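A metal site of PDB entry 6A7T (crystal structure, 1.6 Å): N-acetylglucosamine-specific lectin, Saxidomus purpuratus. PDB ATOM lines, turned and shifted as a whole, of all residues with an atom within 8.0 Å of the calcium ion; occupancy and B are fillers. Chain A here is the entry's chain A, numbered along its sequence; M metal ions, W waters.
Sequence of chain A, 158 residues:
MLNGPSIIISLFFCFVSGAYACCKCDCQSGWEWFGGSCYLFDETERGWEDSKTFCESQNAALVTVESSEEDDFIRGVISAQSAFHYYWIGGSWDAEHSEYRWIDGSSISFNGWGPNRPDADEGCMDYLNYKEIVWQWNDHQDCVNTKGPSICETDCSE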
ATOM      1  N   PHE A  34       3.789  16.714   6.781  1.00  0.00           N
ATOM      2  CA  PHE A  34       3.439  17.839   5.943  1.00  0.00           C
ATOM      3  C   PHE A  34       2.978  17.313   4.594  1.00  0.00           C
ATOM      4  O   PHE A  34       3.638  16.500   3.986  1.00  0.00           O
ATOM      5  CB  PHE A  34       4.633  18.780   5.788  1.00  0.00           C
ATOM      6  CG  PHE A  34       4.357  19.885   4.801  1.00  0.00           C
ATOM      7  CD1 PHE A  34       3.592  20.974   5.197  1.00  0.00           C
ATOM      8  CD2 PHE A  34       4.733  19.777   3.475  1.00  0.00           C
ATOM      9  CE1 PHE A  34       3.266  21.949   4.283  1.00  0.00           C
ATOM     10  CE2 PHE A  34       4.441  20.788   2.573  1.00  0.00           C
ATOM     11  CZ  PHE A  34       3.706  21.853   2.989  1.00  0.00           C
ATOM     12  N   GLY A  35       1.808  17.784   4.104  1.00  0.00           N
ATOM     13  CA  GLY A  35       1.525  17.629   2.676  1.00  0.00           C
ATOM     14  C   GLY A  35       1.376  16.167   2.220  1.00  0.00           C
ATOM     15  O   GLY A  35       1.677  15.856   1.077  1.00  0.00           O
ATOM     16  N   SER A  37       3.005  13.585   3.550  1.00  0.00           N
ATOM     17  CA  SER A  37       4.230  12.801   3.800  1.00  0.00           C
ATOM     18  C   SER A  37       4.693  12.990   5.225  1.00  0.00           C
ATOM     19  O   SER A  37       4.406  13.991   5.849  1.00  0.00           O
ATOM     20  CB  SER A  37       5.347  13.249   2.897  1.00  0.00           C
ATOM     21  OG  SER A  37       5.076  12.899   1.558  1.00  0.00           O
ATOM     22  N   TYR A  39       8.332  13.176   7.439  1.00  0.00           N
ATOM     23  CA  TYR A  39       9.731  13.558   7.260  1.00  0.00           C
ATOM     24  C   TYR A  39      10.537  13.308   8.525  1.00  0.00           C
ATOM     25  O   TYR A  39      10.107  13.629   9.647  1.00  0.00           O
ATOM     26  CB  TYR A  39       9.821  15.041   6.959  1.00  0.00           C
ATOM     27  CG  TYR A  39       9.081  15.473   5.706  1.00  0.00           C
ATOM     28  CD1 TYR A  39       7.705  15.656   5.710  1.00  0.00           C
ATOM     29  CD2 TYR A  39       9.764  15.698   4.519  1.00  0.00           C
ATOM     30  CE1 TYR A  39       7.009  16.009   4.549  1.00  0.00           C
ATOM     31  CE2 TYR A  39       9.100  16.149   3.392  1.00  0.00           C
ATOM     32  CZ  TYR A  39       7.719  16.253   3.389  1.00  0.00           C
ATOM     33  OH  TYR A  39       7.123  16.677   2.231  1.00  0.00           O
ATOM     34  N   LEU A  62      15.557   9.730   0.568  1.00  0.00           N
ATOM     35  CA  LEU A  62      15.936  11.133   0.713  1.00  0.00           C
ATOM     36  C   LEU A  62      14.853  12.019   0.057  1.00  0.00           C
ATOM     37  O   LEU A  62      14.287  11.686  -0.998  1.00  0.00           O
ATOM     38  CB  LEU A  62      17.309  11.356   0.078  1.00  0.00           C
ATOM     39  CG  LEU A  62      18.532  10.890   0.849  1.00  0.00           C
ATOM     40  CD1 LEU A  62      19.746  10.878  -0.061  1.00  0.00           C
ATOM     41  CD2 LEU A  62      18.739  11.761   2.067  1.00  0.00           C
ATOM     42  N   VAL A  63      14.535  13.145   0.737  1.00  0.00           N
ATOM     43  CA  VAL A  63      13.460  14.019   0.361  1.00  0.00           C
ATOM     44  C   VAL A  63      13.601  14.538  -1.062  1.00  0.00           C
ATOM     45  O   VAL A  63      14.661  14.870  -1.491  1.00  0.00           O
ATOM     46  CB  VAL A  63      13.342  15.187   1.361  1.00  0.00           C
ATOM     47  CG1 VAL A  63      14.552  16.096   1.307  1.00  0.00           C
ATOM     48  CG2 VAL A  63      12.047  15.943   1.163  1.00  0.00           C
ATOM     49  N   THR A  64      12.483  14.578  -1.785  1.00  0.00           N
ATOM     50  CA  THR A  64      12.407  15.204  -3.116  1.00  0.00           C
ATOM     51  C   THR A  64      11.441  16.390  -2.979  1.00  0.00           C
ATOM     52  O   THR A  64      10.520  16.298  -2.227  1.00  0.00           O
ATOM     53  CB  THR A  64      11.964  14.175  -4.137  1.00  0.00           C
ATOM     54  OG1 THR A  64      10.676  13.729  -3.721  1.00  0.00           O
ATOM     55  CG2 THR A  64      12.941  13.033  -4.193  1.00  0.00           C
ATOM     56  N   VAL A  65      11.775  17.520  -3.633  1.00  0.00           N
ATOM     57  CA  VAL A  65      11.113  18.814  -3.339  1.00  0.00           C
ATOM     58  C   VAL A  65      10.429  19.310  -4.611  1.00  0.00           C
ATOM     59  O   VAL A  65      11.072  19.946  -5.452  1.00  0.00           O
ATOM     60  CB  VAL A  65      12.084  19.847  -2.761  1.00  0.00           C
ATOM     61  CG1 VAL A  65      11.325  21.102  -2.285  1.00  0.00           C
ATOM     62  CG2 VAL A  65      12.932  19.265  -1.635  1.00  0.00           C
ATOM     63  N   GLU A  66       9.178  18.908  -4.715  1.00  0.00           N
ATOM     64  CA  GLU A  66       8.365  19.091  -5.930  1.00  0.00           C
ATOM     65  C   GLU A  66       7.729  20.466  -6.008  1.00  0.00           C
ATOM     66  O   GLU A  66       7.330  20.882  -7.124  1.00  0.00           O
ATOM     67  CB  GLU A  66       7.271  18.043  -5.986  1.00  0.00           C
ATOM     68  CG  GLU A  66       7.808  16.663  -6.365  1.00  0.00           C
ATOM     69  CD  GLU A  66       8.283  15.778  -5.210  1.00  0.00           C
ATOM     70  OE1 GLU A  66       7.987  16.094  -4.008  1.00  0.00           O
ATOM     71  OE2 GLU A  66       8.966  14.784  -5.523  1.00  0.00           O
ATOM     72  N   SER A  67       7.559  21.136  -4.854  1.00  0.00           N
ATOM     73  CA  SER A  67       6.719  22.344  -4.791  1.00  0.00           C
ATOM     74  C   SER A  67       7.386  23.380  -3.891  1.00  0.00           C
ATOM     75  O   SER A  67       8.168  23.007  -2.996  1.00  0.00           O
ATOM     76  CB  SER A  67       5.319  22.022  -4.344  1.00  0.00           C
ATOM     77  OG  SER A  67       5.250  21.651  -2.958  1.00  0.00           O
ATOM     78  N   GLU A  70       6.494  22.829  -0.281  1.00  0.00           N
ATOM     79  CA  GLU A  70       7.303  21.803   0.447  1.00  0.00           C
ATOM     80  C   GLU A  70       8.645  22.401   0.822  1.00  0.00           C
ATOM     81  O   GLU A  70       9.196  22.129   1.913  1.00  0.00           O
ATOM     82  CB  GLU A  70       7.448  20.538  -0.405  1.00  0.00           C
ATOM     83  CG  GLU A  70       8.131  19.361   0.325  1.00  0.00           C
ATOM     84  CD  GLU A  70       8.265  18.101  -0.521  1.00  0.00           C
ATOM     85  OE1 GLU A  70       8.509  17.052   0.051  1.00  0.00           O
ATOM     86  OE2 GLU A  70       8.058  18.145  -1.784  1.00  0.00           O
ATOM     87  N   ASP A  71       9.182  23.201  -0.089  1.00  0.00           N
ATOM     88  CA  ASP A  71      10.440  23.888   0.111  1.00  0.00           C
ATOM     89  C   ASP A  71      10.332  24.745   1.375  1.00  0.00           C
ATOM     90  O   ASP A  71      11.218  24.732   2.222  1.00  0.00           O
ATOM     91  CB  ASP A  71      10.790  24.717  -1.111  1.00  0.00           C
ATOM     92  CG  ASP A  71      12.100  25.461  -1.010  1.00  0.00           C
ATOM     93  OD1 ASP A  71      13.145  24.827  -0.943  1.00  0.00           O
ATOM     94  OD2 ASP A  71      12.030  26.750  -1.044  1.00  0.00           O
ATOM     95  N   ILE A  74      10.329  22.668   4.577  1.00  0.00           N
ATOM     96  CA  ILE A  74      11.648  22.159   4.936  1.00  0.00           C
ATOM     97  C   ILE A  74      12.482  23.289   5.529  1.00  0.00           C
ATOM     98  O   ILE A  74      13.124  23.106   6.556  1.00  0.00           O
ATOM     99  CB  ILE A  74      12.324  21.504   3.721  1.00  0.00           C
ATOM    100  CG1 ILE A  74      11.583  20.229   3.330  1.00  0.00           C
ATOM    101  CG2 ILE A  74      13.794  21.264   3.992  1.00  0.00           C
ATOM    102  CD1 ILE A  74      11.894  19.716   1.949  1.00  0.00           C
ATOM    103  N   TRP A 102      15.692  14.334  -9.328  1.00  0.00           N
ATOM    104  CA  TRP A 102      15.343  13.719  -8.050  1.00  0.00           C
ATOM    105  C   TRP A 102      15.644  12.230  -8.144  1.00  0.00           C
ATOM    106  O   TRP A 102      15.644  11.655  -9.209  1.00  0.00           O
ATOM    107  CB  TRP A 102      13.884  13.962  -7.681  1.00  0.00           C
ATOM    108  CG  TRP A 102      13.590  15.421  -7.500  1.00  0.00           C
ATOM    109  CD1 TRP A 102      12.690  16.163  -8.205  1.00  0.00           C
ATOM    110  CD2 TRP A 102      14.170  16.313  -6.547  1.00  0.00           C
ATOM    111  NE1 TRP A 102      12.668  17.466  -7.769  1.00  0.00           N
ATOM    112  CE2 TRP A 102      13.581  17.587  -6.770  1.00  0.00           C
ATOM    113  CE3 TRP A 102      15.154  16.174  -5.559  1.00  0.00           C
ATOM    114  CZ2 TRP A 102      13.934  18.683  -5.998  1.00  0.00           C
ATOM    115  CZ3 TRP A 102      15.538  17.274  -4.839  1.00  0.00           C
ATOM    116  CH2 TRP A 102      14.930  18.528  -5.074  1.00  0.00           C
ATOM    117  N   ASP A 104      13.966   9.618  -7.501  1.00  0.00           N
ATOM    118  CA  ASP A 104      12.948   8.800  -8.178  1.00  0.00           C
ATOM    119  C   ASP A 104      13.012   8.918  -9.718  1.00  0.00           C
ATOM    120  O   ASP A 104      12.131   8.343 -10.417  1.00  0.00           O
ATOM    121  CB  ASP A 104      11.523   9.144  -7.761  1.00  0.00           C
ATOM    122  CG  ASP A 104      11.098  10.590  -7.998  1.00  0.00           C
ATOM    123  OD1 ASP A 104      11.862  11.367  -8.568  1.00  0.00           O
ATOM    124  OD2 ASP A 104       9.967  10.915  -7.566  1.00  0.00           O
ATOM    125  N   GLU A 153      11.951  11.302   3.452  1.00  0.00           N
ATOM    126  CA  GLU A 153      10.531  11.522   3.189  1.00  0.00           C
ATOM    127  C   GLU A 153       9.873  10.152   2.960  1.00  0.00           C
ATOM    128  O   GLU A 153      10.397   9.370   2.208  1.00  0.00           O
ATOM    129  CB  GLU A 153      10.367  12.463   1.995  1.00  0.00           C
ATOM    130  CG  GLU A 153       8.914  12.784   1.637  1.00  0.00           C
ATOM    131  CD  GLU A 153       8.701  13.637   0.393  1.00  0.00           C
ATOM    132  OE1 GLU A 153       9.658  13.817  -0.436  1.00  0.00           O
ATOM    133  OE2 GLU A 153       7.561  14.082   0.222  1.00  0.00           O
ATOM    134  N   THR A 154       8.703   9.911   3.570  1.00  0.00           N
ATOM    135  CA  THR A 154       7.914   8.716   3.240  1.00  0.00           C
ATOM    136  C   THR A 154       6.473   9.148   2.945  1.00  0.00           C
ATOM    137  O   THR A 154       5.959  10.118   3.539  1.00  0.00           O
ATOM    138  CB  THR A 154       7.934   7.675   4.372  1.00  0.00           C
ATOM    139  OG1 THR A 154       7.232   6.513   3.932  1.00  0.00           O
ATOM    140  CG2 THR A 154       7.362   8.209   5.664  1.00  0.00           C
HETATM  141 CA    CA M   1       8.314  15.508  -1.789  1.00  0.00          CA
HETATM  142  O   HOH W   1       7.708  13.340  -2.860  1.00  0.00           O
HETATM  143  O   HOH W   2       5.853  15.742  -1.867  1.00  0.00           O
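The side-chain hydroxyl (OH) of Tyr 39 sits close to the side-chain carboxylate (OE1) of Glu 70 (2.6 Å). OG of Ser 67 lies within hydrogen-bond range of N of Glu 70. The side-chain carboxylate of Glu 153 sits close to the side-chain hydroxyl of Tyr 39, 3.3 Å away. The side-chain hydroxyl of Ser 37 sits close to the side-chain carboxylate of Glu 153 (3.1 Å).
The calcium ion is bound by the side-chain carboxylate (OE1) of Glu 66 (2.3 Å), the backbone carbonyl oxygen (O) of Thr 64 (2.4 Å), the side-chain carboxylate (OE1) of Glu 70 (2.4 Å), water W2 (2.5 Å), water W1 (2.5 Å), the side-chain carboxylate (OE1) of Glu 153 (2.5 Å), the side-chain carboxylate (OE2) of Glu 153 (2.6 Å) and the side-chain carboxylate (OE2) of Glu 70 (2.6 Å).
Within 4 Å of the calcium ion: Thr 64, Glu 66, Glu 70 and Glu 153. The nearest printed residue that does not touch the calcium ion is Tyr 39 (4.4 Å).
Water W1 lies within hydrogen-bond range of the side-chain hydroxyl (OG1) of Thr 64 (3.1 Å) and the side-chain carboxylate (OE2) of Glu 66 (3.3 Å).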
